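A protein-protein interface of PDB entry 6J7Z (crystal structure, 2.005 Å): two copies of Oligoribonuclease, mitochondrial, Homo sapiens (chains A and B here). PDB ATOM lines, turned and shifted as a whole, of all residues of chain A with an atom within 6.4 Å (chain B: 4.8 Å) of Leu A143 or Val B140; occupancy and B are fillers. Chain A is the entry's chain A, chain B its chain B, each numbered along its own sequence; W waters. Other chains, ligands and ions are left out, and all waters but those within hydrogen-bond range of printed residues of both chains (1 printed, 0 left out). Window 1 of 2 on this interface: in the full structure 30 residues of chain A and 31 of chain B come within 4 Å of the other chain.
Among the printed residues, pairs that only touch across the chains: Ile A134 with Asp B136 (3.6 Å), Thr A139 with Ile B135 (3.7 Å), Val A140 with Leu B143 (3.8 Å), Leu A143 with Val B140 (3.8 Å), Arg A146 with Met B11 (3.6 Å), Tyr A148 with Phe B183 (3.4 Å), Ile A182 with Phe B183 (3.5 Å), Phe A183 with Ile B182 (3.5 Å) and Phe A183 with Phe B183 (3.7 Å).
OD1 of Asp B136 sits at hydrogen-bond distance from N of Ser B138 (2.9 Å).
The side-chain carboxylate (OE2) of Glu A142 lies within salt-bridge range of the guanidinium group (NH1) of Arg A146 (2.4 Å).
SG of Cys A144 is in hydrogen-bond range of O of Tyr A148 (3.7 Å).
Val A140 touches Leu B143, and with the chains exchanged Leu A143 touches Val B140.
Ile A182 touches Phe B183, and with the chains exchanged Phe A183 touches Ile B182.
Phe A183 touches its own counterpart, Phe B183.
Of the 11 pairs that touch across the chains among the printed residues, 5 have their exchanged pair printed and touching as well.
Printed residues of chain B within 4 Å of Ile A134: Asp B136 and Thr B139.
Val B140 touches just one residue of chain A: Leu A143.
Of the printed residues of chain A, Leu B143 touches Val A140 (3.8 Å).
The nearest printed residue of chain B that does not touch Thr A139 is Val B140 (4.3 Å).
Printed residues of chain A that touch a printed residue of chain B: Ile A134, Thr A139, Val A140, Leu A143, Arg A146, Tyr A148, Ile A182 and Phe A183.
Hydrophobic or aromatic side chains of chain A that line the printed part of chain B: Ile A134, Val A140, Leu A143, Tyr A148, Ile A182 and Phe A183.
Printed residues of chain B that touch a printed residue of chain A: Met B11, Ile B135, Asp B136, Thr B139, Val B140, Leu B143, Ile B182 and Phe B183.
Among the printed residues, 11 pairs touch across the chains.
Among the printed residues, no Asp or Glu carboxylate lies within 4 Å of a Lys or Arg side-chain nitrogen of the other chain.
Water W1 bridges OD2 of Asp B136 and N of Ile A134.
OG1 of Thr A139 is in hydrogen-bond range of N of Asp B136 (2.9 Å).
O of Ile A134 lies within hydrogen-bond range of OG1 of Thr B139 (2.9 Å).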
ATOM      1  N   ILE A 134      14.850 -11.040  -6.432  1.00  0.00           N
ATOM      2  CA  ILE A 134      15.684 -11.017  -5.242  1.00  0.00           C
ATOM      3  C   ILE A 134      15.284  -9.827  -4.385  1.00  0.00           C
ATOM      4  O   ILE A 134      14.697  -8.852  -4.859  1.00  0.00           O
ATOM      5  CB  ILE A 134      17.190 -10.942  -5.574  1.00  0.00           C
ATOM      6  CG1 ILE A 134      17.528  -9.595  -6.220  1.00  0.00           C
ATOM      7  CG2 ILE A 134      17.594 -12.086  -6.479  1.00  0.00           C
ATOM      8  CD1 ILE A 134      18.988  -9.436  -6.579  1.00  0.00           C
ATOM      9  N   SER A 138      21.259  -4.046  -0.728  1.00  0.00           N
ATOM     10  CA  SER A 138      22.112  -2.986  -1.258  1.00  0.00           C
ATOM     11  C   SER A 138      21.320  -1.993  -2.100  1.00  0.00           C
ATOM     12  O   SER A 138      21.682  -0.814  -2.170  1.00  0.00           O
ATOM     13  CB  SER A 138      23.253  -3.589  -2.077  1.00  0.00           C
ATOM     14  OG  SER A 138      24.184  -4.245  -1.233  1.00  0.00           O
ATOM     15  N   THR A 139      20.238  -2.443  -2.737  1.00  0.00           N
ATOM     16  CA  THR A 139      19.376  -1.521  -3.470  1.00  0.00           C
ATOM     17  C   THR A 139      18.739  -0.507  -2.525  1.00  0.00           C
ATOM     18  O   THR A 139      18.762   0.706  -2.780  1.00  0.00           O
ATOM     19  CB  THR A 139      18.304  -2.304  -4.230  1.00  0.00           C
ATOM     20  OG1 THR A 139      18.888  -2.917  -5.386  1.00  0.00           O
ATOM     21  CG2 THR A 139      17.170  -1.388  -4.664  1.00  0.00           C
ATOM     22  N   VAL A 140      18.171  -0.991  -1.417  1.00  0.00           N
ATOM     23  CA  VAL A 140      17.597  -0.093  -0.422  1.00  0.00           C
ATOM     24  C   VAL A 140      18.677   0.784   0.193  1.00  0.00           C
ATOM     25  O   VAL A 140      18.425   1.943   0.534  1.00  0.00           O
ATOM     26  CB  VAL A 140      16.840  -0.900   0.650  1.00  0.00           C
ATOM     27  CG1 VAL A 140      16.078   0.033   1.578  1.00  0.00           C
ATOM     28  CG2 VAL A 140      15.894  -1.893  -0.006  1.00  0.00           C
ATOM     29  N   LYS A 141      19.896   0.256   0.331  1.00  0.00           N
ATOM     30  CA  LYS A 141      20.998   1.056   0.856  1.00  0.00           C
ATOM     31  C   LYS A 141      21.329   2.217  -0.074  1.00  0.00           C
ATOM     32  O   LYS A 141      21.536   3.348   0.381  1.00  0.00           O
ATOM     33  CB  LYS A 141      22.226   0.171   1.072  1.00  0.00           C
ATOM     34  CG  LYS A 141      23.480   0.922   1.494  1.00  0.00           C
ATOM     35  CD  LYS A 141      24.712   0.038   1.365  1.00  0.00           C
ATOM     36  CE  LYS A 141      25.966   0.756   1.838  1.00  0.00           C
ATOM     37  NZ  LYS A 141      25.987   0.924   3.317  1.00  0.00           N
ATOM     38  N   GLU A 142      21.385   1.954  -1.380  1.00  0.00           N
ATOM     39  CA  GLU A 142      21.640   3.021  -2.344  1.00  0.00           C
ATOM     40  C   GLU A 142      20.511   4.044  -2.344  1.00  0.00           C
ATOM     41  O   GLU A 142      20.755   5.257  -2.402  1.00  0.00           O
ATOM     42  CB  GLU A 142      21.828   2.428  -3.741  1.00  0.00           C
ATOM     43  CG  GLU A 142      23.224   1.893  -4.006  1.00  0.00           C
ATOM     44  CD  GLU A 142      24.293   2.954  -3.838  1.00  0.00           C
ATOM     45  OE1 GLU A 142      25.283   2.695  -3.122  1.00  0.00           O
ATOM     46  OE2 GLU A 142      24.143   4.048  -4.421  1.00  0.00           O
ATOM     47  N   LEU A 143      19.263   3.571  -2.278  1.00  0.00           N
ATOM     48  CA  LEU A 143      18.132   4.495  -2.242  1.00  0.00           C
ATOM     49  C   LEU A 143      18.150   5.344  -0.975  1.00  0.00           C
ATOM     50  O   LEU A 143      17.790   6.524  -1.011  1.00  0.00           O
ATOM     51  CB  LEU A 143      16.820   3.723  -2.361  1.00  0.00           C
ATOM     52  CG  LEU A 143      16.583   3.031  -3.706  1.00  0.00           C
ATOM     53  CD1 LEU A 143      15.211   2.378  -3.736  1.00  0.00           C
ATOM     54  CD2 LEU A 143      16.741   4.015  -4.859  1.00  0.00           C
ATOM     55  N   CYS A 144      18.572   4.764   0.151  1.00  0.00           N
ATOM     56  CA  CYS A 144      18.680   5.529   1.388  1.00  0.00           C
ATOM     57  C   CYS A 144      19.816   6.540   1.314  1.00  0.00           C
ATOM     58  O   CYS A 144      19.684   7.668   1.799  1.00  0.00           O
ATOM     59  CB  CYS A 144      18.881   4.580   2.572  1.00  0.00           C
ATOM     60  SG  CYS A 144      18.998   5.390   4.185  1.00  0.00           S
ATOM     61  N   ARG A 145      20.940   6.149   0.711  1.00  0.00           N
ATOM     62  CA  ARG A 145      22.054   7.076   0.546  1.00  0.00           C
ATOM     63  C   ARG A 145      21.655   8.267  -0.316  1.00  0.00           C
ATOM     64  O   ARG A 145      22.050   9.405  -0.038  1.00  0.00           O
ATOM     65  CB  ARG A 145      23.251   6.348  -0.067  1.00  0.00           C
ATOM     66  CG  ARG A 145      24.549   7.134  -0.028  1.00  0.00           C
ATOM     67  CD  ARG A 145      25.685   6.350  -0.665  1.00  0.00           C
ATOM     68  NE  ARG A 145      25.457   6.113  -2.088  1.00  0.00           N
ATOM     69  CZ  ARG A 145      25.751   6.985  -3.047  1.00  0.00           C
ATOM     70  NH1 ARG A 145      26.287   8.157  -2.737  1.00  0.00           N
ATOM     71  NH2 ARG A 145      25.511   6.686  -4.315  1.00  0.00           N
ATOM     72  N   ARG A 146      20.860   8.025  -1.360  1.00  0.00           N
ATOM     73  CA  ARG A 146      20.482   9.107  -2.263  1.00  0.00           C
ATOM     74  C   ARG A 146      19.364   9.970  -1.685  1.00  0.00           C
ATOM     75  O   ARG A 146      19.445  11.203  -1.712  1.00  0.00           O
ATOM     76  CB  ARG A 146      20.060   8.535  -3.616  1.00  0.00           C
ATOM     77  CG  ARG A 146      21.216   8.042  -4.461  1.00  0.00           C
ATOM     78  CD  ARG A 146      20.723   7.383  -5.736  1.00  0.00           C
ATOM     79  NE  ARG A 146      21.771   7.308  -6.749  1.00  0.00           N
ATOM     80  CZ  ARG A 146      22.726   6.385  -6.765  1.00  0.00           C
ATOM     81  NH1 ARG A 146      22.768   5.454  -5.821  1.00  0.00           N
ATOM     82  NH2 ARG A 146      23.641   6.393  -7.725  1.00  0.00           N
ATOM     83  N   TRP A 147      18.312   9.342  -1.164  1.00  0.00           N
ATOM     84  CA  TRP A 147      17.106  10.062  -0.778  1.00  0.00           C
ATOM     85  C   TRP A 147      17.053  10.434   0.697  1.00  0.00           C
ATOM     86  O   TRP A 147      16.334  11.374   1.051  1.00  0.00           O
ATOM     87  CB  TRP A 147      15.866   9.232  -1.128  1.00  0.00           C
ATOM     88  CG  TRP A 147      15.740   8.910  -2.591  1.00  0.00           C
ATOM     89  CD1 TRP A 147      16.391   9.516  -3.627  1.00  0.00           C
ATOM     90  CD2 TRP A 147      14.908   7.901  -3.177  1.00  0.00           C
ATOM     91  NE1 TRP A 147      16.016   8.948  -4.821  1.00  0.00           N
ATOM     92  CE2 TRP A 147      15.106   7.954  -4.571  1.00  0.00           C
ATOM     93  CE3 TRP A 147      14.015   6.959  -2.658  1.00  0.00           C
ATOM     94  CZ2 TRP A 147      14.444   7.101  -5.452  1.00  0.00           C
ATOM     95  CZ3 TRP A 147      13.358   6.113  -3.533  1.00  0.00           C
ATOM     96  CH2 TRP A 147      13.577   6.190  -4.914  1.00  0.00           C
ATOM     97  N   TYR A 148      17.786   9.733   1.563  1.00  0.00           N
ATOM     98  CA  TYR A 148      17.740   9.972   3.010  1.00  0.00           C
ATOM     99  C   TYR A 148      19.151   9.943   3.583  1.00  0.00           C
ATOM    100  O   TYR A 148      19.498   9.066   4.382  1.00  0.00           O
ATOM    101  CB  TYR A 148      16.847   8.936   3.697  1.00  0.00           C
ATOM    102  CG  TYR A 148      15.421   8.929   3.194  1.00  0.00           C
ATOM    103  CD1 TYR A 148      14.451   9.725   3.789  1.00  0.00           C
ATOM    104  CD2 TYR A 148      15.046   8.130   2.121  1.00  0.00           C
ATOM    105  CE1 TYR A 148      13.149   9.725   3.332  1.00  0.00           C
ATOM    106  CE2 TYR A 148      13.745   8.125   1.655  1.00  0.00           C
ATOM    107  CZ  TYR A 148      12.801   8.924   2.265  1.00  0.00           C
ATOM    108  OH  TYR A 148      11.503   8.923   1.808  1.00  0.00           O
ATOM    109  N   ILE A 182      13.106   4.988   6.855  1.00  0.00           N
ATOM    110  CA  ILE A 182      12.929   5.697   5.590  1.00  0.00           C
ATOM    111  C   ILE A 182      11.645   5.283   4.880  1.00  0.00           C
ATOM    112  O   ILE A 182      11.291   5.851   3.841  1.00  0.00           O
ATOM    113  CB  ILE A 182      14.141   5.510   4.660  1.00  0.00           C
ATOM    114  CG1 ILE A 182      14.202   4.078   4.126  1.00  0.00           C
ATOM    115  CG2 ILE A 182      15.433   5.901   5.365  1.00  0.00           C
ATOM    116  CD1 ILE A 182      15.226   3.888   3.033  1.00  0.00           C
ATOM    117  N   PHE A 183      10.936   4.302   5.423  1.00  0.00           N
ATOM    118  CA  PHE A 183       9.673   3.875   4.843  1.00  0.00           C
ATOM    119  C   PHE A 183       8.503   4.508   5.587  1.00  0.00           C
ATOM    120  O   PHE A 183       8.609   4.886   6.756  1.00  0.00           O
ATOM    121  CB  PHE A 183       9.554   2.349   4.854  1.00  0.00           C
ATOM    122  CG  PHE A 183      10.300   1.673   3.734  1.00  0.00           C
ATOM    123  CD1 PHE A 183      11.649   1.383   3.856  1.00  0.00           C
ATOM    124  CD2 PHE A 183       9.650   1.333   2.558  1.00  0.00           C
ATOM    125  CE1 PHE A 183      12.337   0.760   2.827  1.00  0.00           C
ATOM    126  CE2 PHE A 183      10.331   0.712   1.527  1.00  0.00           C
ATOM    127  CZ  PHE A 183      11.675   0.425   1.661  1.00  0.00           C
ATOM    128  N   MET B  11      21.908   7.487 -12.482  1.00  0.00           N
ATOM    129  CA  MET B  11      21.573   6.082 -12.660  1.00  0.00           C
ATOM    130  C   MET B  11      21.496   5.752 -14.144  1.00  0.00           C
ATOM    131  O   MET B  11      20.933   6.527 -14.934  1.00  0.00           O
ATOM    132  CB  MET B  11      20.239   5.731 -11.998  1.00  0.00           C
ATOM    133  CG  MET B  11      20.097   6.169 -10.554  1.00  0.00           C
ATOM    134  SD  MET B  11      18.467   5.724  -9.925  1.00  0.00           S
ATOM    135  CE  MET B  11      18.427   6.628  -8.382  1.00  0.00           C
ATOM    136  N   ILE B 135      20.565  -1.019  -8.766  1.00  0.00           N
ATOM    137  CA  ILE B 135      19.334  -0.503  -8.178  1.00  0.00           C
ATOM    138  C   ILE B 135      18.204  -1.333  -8.773  1.00  0.00           C
ATOM    139  O   ILE B 135      17.748  -1.074  -9.894  1.00  0.00           O
ATOM    140  CB  ILE B 135      19.140   0.995  -8.443  1.00  0.00           C
ATOM    141  CG1 ILE B 135      20.256   1.792  -7.765  1.00  0.00           C
ATOM    142  CG2 ILE B 135      17.779   1.459  -7.940  1.00  0.00           C
ATOM    143  CD1 ILE B 135      20.058   3.288  -7.813  1.00  0.00           C
ATOM    144  N   ASP B 136      17.764  -2.348  -8.034  1.00  0.00           N
ATOM    145  CA  ASP B 136      16.763  -3.293  -8.515  1.00  0.00           C
ATOM    146  C   ASP B 136      15.388  -2.825  -8.059  1.00  0.00           C
ATOM    147  O   ASP B 136      15.070  -2.874  -6.866  1.00  0.00           O
ATOM    148  CB  ASP B 136      17.070  -4.699  -8.007  1.00  0.00           C
ATOM    149  CG  ASP B 136      16.157  -5.756  -8.605  1.00  0.00           C
ATOM    150  OD1 ASP B 136      15.263  -5.404  -9.405  1.00  0.00           O
ATOM    151  OD2 ASP B 136      16.334  -6.945  -8.269  1.00  0.00           O
ATOM    152  N   VAL B 137      14.571  -2.374  -9.014  1.00  0.00           N
ATOM    153  CA  VAL B 137      13.214  -1.944  -8.696  1.00  0.00           C
ATOM    154  C   VAL B 137      12.389  -3.105  -8.159  1.00  0.00           C
ATOM    155  O   VAL B 137      11.477  -2.905  -7.348  1.00  0.00           O
ATOM    156  CB  VAL B 137      12.557  -1.310  -9.940  1.00  0.00           C
ATOM    157  CG1 VAL B 137      11.144  -0.827  -9.624  1.00  0.00           C
ATOM    158  CG2 VAL B 137      13.408  -0.165 -10.455  1.00  0.00           C
ATOM    159  N   SER B 138      12.697  -4.334  -8.583  1.00  0.00           N
ATOM    160  CA  SER B 138      11.908  -5.481  -8.148  1.00  0.00           C
ATOM    161  C   SER B 138      12.094  -5.771  -6.663  1.00  0.00           C
ATOM    162  O   SER B 138      11.186  -6.317  -6.025  1.00  0.00           O
ATOM    163  CB  SER B 138      12.263  -6.709  -8.985  1.00  0.00           C
ATOM    164  OG  SER B 138      11.778  -6.571 -10.309  1.00  0.00           O
ATOM    165  N   THR B 139      13.247  -5.412  -6.095  1.00  0.00           N
ATOM    166  CA  THR B 139      13.413  -5.500  -4.647  1.00  0.00           C
ATOM    167  C   THR B 139      12.397  -4.615  -3.932  1.00  0.00           C
ATOM    168  O   THR B 139      11.711  -5.055  -2.998  1.00  0.00           O
ATOM    169  CB  THR B 139      14.839  -5.104  -4.258  1.00  0.00           C
ATOM    170  OG1 THR B 139      15.755  -6.126  -4.671  1.00  0.00           O
ATOM    171  CG2 THR B 139      14.951  -4.906  -2.753  1.00  0.00           C
ATOM    172  N   VAL B 140      12.285  -3.359  -4.371  1.00  0.00           N
ATOM    173  CA  VAL B 140      11.290  -2.454  -3.806  1.00  0.00           C
ATOM    174  C   VAL B 140       9.884  -2.965  -4.082  1.00  0.00           C
ATOM    175  O   VAL B 140       8.979  -2.783  -3.262  1.00  0.00           O
ATOM    176  CB  VAL B 140      11.489  -1.029  -4.359  1.00  0.00           C
ATOM    177  CG1 VAL B 140      10.619  -0.037  -3.603  1.00  0.00           C
ATOM    178  CG2 VAL B 140      12.955  -0.633  -4.280  1.00  0.00           C
ATOM    179  N   LYS B 141       9.678  -3.624  -5.224  1.00  0.00           N
ATOM    180  CA  LYS B 141       8.361  -4.165  -5.545  1.00  0.00           C
ATOM    181  C   LYS B 141       7.961  -5.256  -4.559  1.00  0.00           C
ATOM    182  O   LYS B 141       6.830  -5.278  -4.062  1.00  0.00           O
ATOM    183  CB  LYS B 141       8.356  -4.702  -6.977  1.00  0.00           C
ATOM    184  CG  LYS B 141       7.134  -5.532  -7.332  1.00  0.00           C
ATOM    185  CD  LYS B 141       7.482  -6.616  -8.341  1.00  0.00           C
ATOM    186  CE  LYS B 141       8.022  -6.020  -9.632  1.00  0.00           C
ATOM    187  NZ  LYS B 141       6.976  -5.270 -10.381  1.00  0.00           N
ATOM    188  N   GLU B 142       8.883  -6.174  -4.268  1.00  0.00           N
ATOM    189  CA  GLU B 142       8.601  -7.231  -3.300  1.00  0.00           C
ATOM    190  C   GLU B 142       8.393  -6.659  -1.901  1.00  0.00           C
ATOM    191  O   GLU B 142       7.477  -7.079  -1.178  1.00  0.00           O
ATOM    192  CB  GLU B 142       9.734  -8.257  -3.306  1.00  0.00           C
ATOM    193  CG  GLU B 142       9.774  -9.119  -4.558  1.00  0.00           C
ATOM    194  CD  GLU B 142       8.526  -9.967  -4.714  1.00  0.00           C
ATOM    195  OE1 GLU B 142       8.094 -10.576  -3.714  1.00  0.00           O
ATOM    196  OE2 GLU B 142       7.974 -10.020  -5.833  1.00  0.00           O
ATOM    197  N   LEU B 143       9.224  -5.688  -1.510  1.00  0.00           N
ATOM    198  CA  LEU B 143       9.051  -5.062  -0.202  1.00  0.00           C
ATOM    199  C   LEU B 143       7.709  -4.346  -0.103  1.00  0.00           C
ATOM    200  O   LEU B 143       7.067  -4.363   0.952  1.00  0.00           O
ATOM    201  CB  LEU B 143      10.198  -4.093   0.074  1.00  0.00           C
ATOM    202  CG  LEU B 143      11.571  -4.736   0.258  1.00  0.00           C
ATOM    203  CD1 LEU B 143      12.609  -3.676   0.581  1.00  0.00           C
ATOM    204  CD2 LEU B 143      11.524  -5.803   1.344  1.00  0.00           C
ATOM    205  N   CYS B 144       7.269  -3.711  -1.191  1.00  0.00           N
ATOM    206  CA  CYS B 144       5.977  -3.037  -1.191  1.00  0.00           C
ATOM    207  C   CYS B 144       4.836  -4.042  -1.129  1.00  0.00           C
ATOM    208  O   CYS B 144       3.850  -3.827  -0.415  1.00  0.00           O
ATOM    209  CB  CYS B 144       5.852  -2.155  -2.435  1.00  0.00           C
ATOM    210  SG  CYS B 144       4.283  -1.279  -2.598  1.00  0.00           S
ATOM    211  N   LEU B 175       9.322   2.752  -9.846  1.00  0.00           N
ATOM    212  CA  LEU B 175      10.123   3.223  -8.719  1.00  0.00           C
ATOM    213  C   LEU B 175       9.645   4.589  -8.234  1.00  0.00           C
ATOM    214  O   LEU B 175       9.659   4.869  -7.027  1.00  0.00           O
ATOM    215  CB  LEU B 175      11.603   3.277  -9.093  1.00  0.00           C
ATOM    216  CG  LEU B 175      12.519   3.645  -7.923  1.00  0.00           C
ATOM    217  CD1 LEU B 175      12.294   2.706  -6.741  1.00  0.00           C
ATOM    218  CD2 LEU B 175      13.976   3.635  -8.348  1.00  0.00           C
ATOM    219  N   TYR B 178       6.667   4.046  -6.071  1.00  0.00           N
ATOM    220  CA  TYR B 178       7.080   3.541  -4.765  1.00  0.00           C
ATOM    221  C   TYR B 178       7.603   4.668  -3.882  1.00  0.00           C
ATOM    222  O   TYR B 178       7.230   4.771  -2.708  1.00  0.00           O
ATOM    223  CB  TYR B 178       8.132   2.443  -4.925  1.00  0.00           C
ATOM    224  CG  TYR B 178       7.580   1.177  -5.532  1.00  0.00           C
ATOM    225  CD1 TYR B 178       6.275   0.776  -5.279  1.00  0.00           C
ATOM    226  CD2 TYR B 178       8.359   0.388  -6.365  1.00  0.00           C
ATOM    227  CE1 TYR B 178       5.761  -0.379  -5.836  1.00  0.00           C
ATOM    228  CE2 TYR B 178       7.857  -0.769  -6.925  1.00  0.00           C
ATOM    229  CZ  TYR B 178       6.557  -1.146  -6.660  1.00  0.00           C
ATOM    230  OH  TYR B 178       6.052  -2.296  -7.219  1.00  0.00           O
ATOM    231  N   ILE B 182       5.277   4.864  -0.572  1.00  0.00           N
ATOM    232  CA  ILE B 182       5.613   3.990   0.552  1.00  0.00           C
ATOM    233  C   ILE B 182       6.866   4.455   1.284  1.00  0.00           C
ATOM    234  O   ILE B 182       7.226   3.893   2.325  1.00  0.00           O
ATOM    235  CB  ILE B 182       5.774   2.524   0.099  1.00  0.00           C
ATOM    236  CG1 ILE B 182       7.056   2.347  -0.716  1.00  0.00           C
ATOM    237  CG2 ILE B 182       4.550   2.058  -0.679  1.00  0.00           C
ATOM    238  CD1 ILE B 182       7.413   0.901  -0.970  1.00  0.00           C
ATOM    239  N   PHE B 183       7.544   5.469   0.759  1.00  0.00           N
ATOM    240  CA  PHE B 183       8.722   6.001   1.428  1.00  0.00           C
ATOM    241  C   PHE B 183       8.345   7.200   2.288  1.00  0.00           C
ATOM    242  O   PHE B 183       7.350   7.884   2.033  1.00  0.00           O
ATOM    243  CB  PHE B 183       9.800   6.386   0.415  1.00  0.00           C
ATOM    244  CG  PHE B 183      10.623   5.221  -0.063  1.00  0.00           C
ATOM    245  CD1 PHE B 183      10.172   4.416  -1.096  1.00  0.00           C
ATOM    246  CD2 PHE B 183      11.840   4.925   0.531  1.00  0.00           C
ATOM    247  CE1 PHE B 183      10.925   3.341  -1.535  1.00  0.00           C
ATOM    248  CE2 PHE B 183      12.597   3.850   0.096  1.00  0.00           C
ATOM    249  CZ  PHE B 183      12.138   3.057  -0.938  1.00  0.00           C
HETATM  250  O   HOH W   1      14.684  -8.838  -8.495  1.00  0.00           O
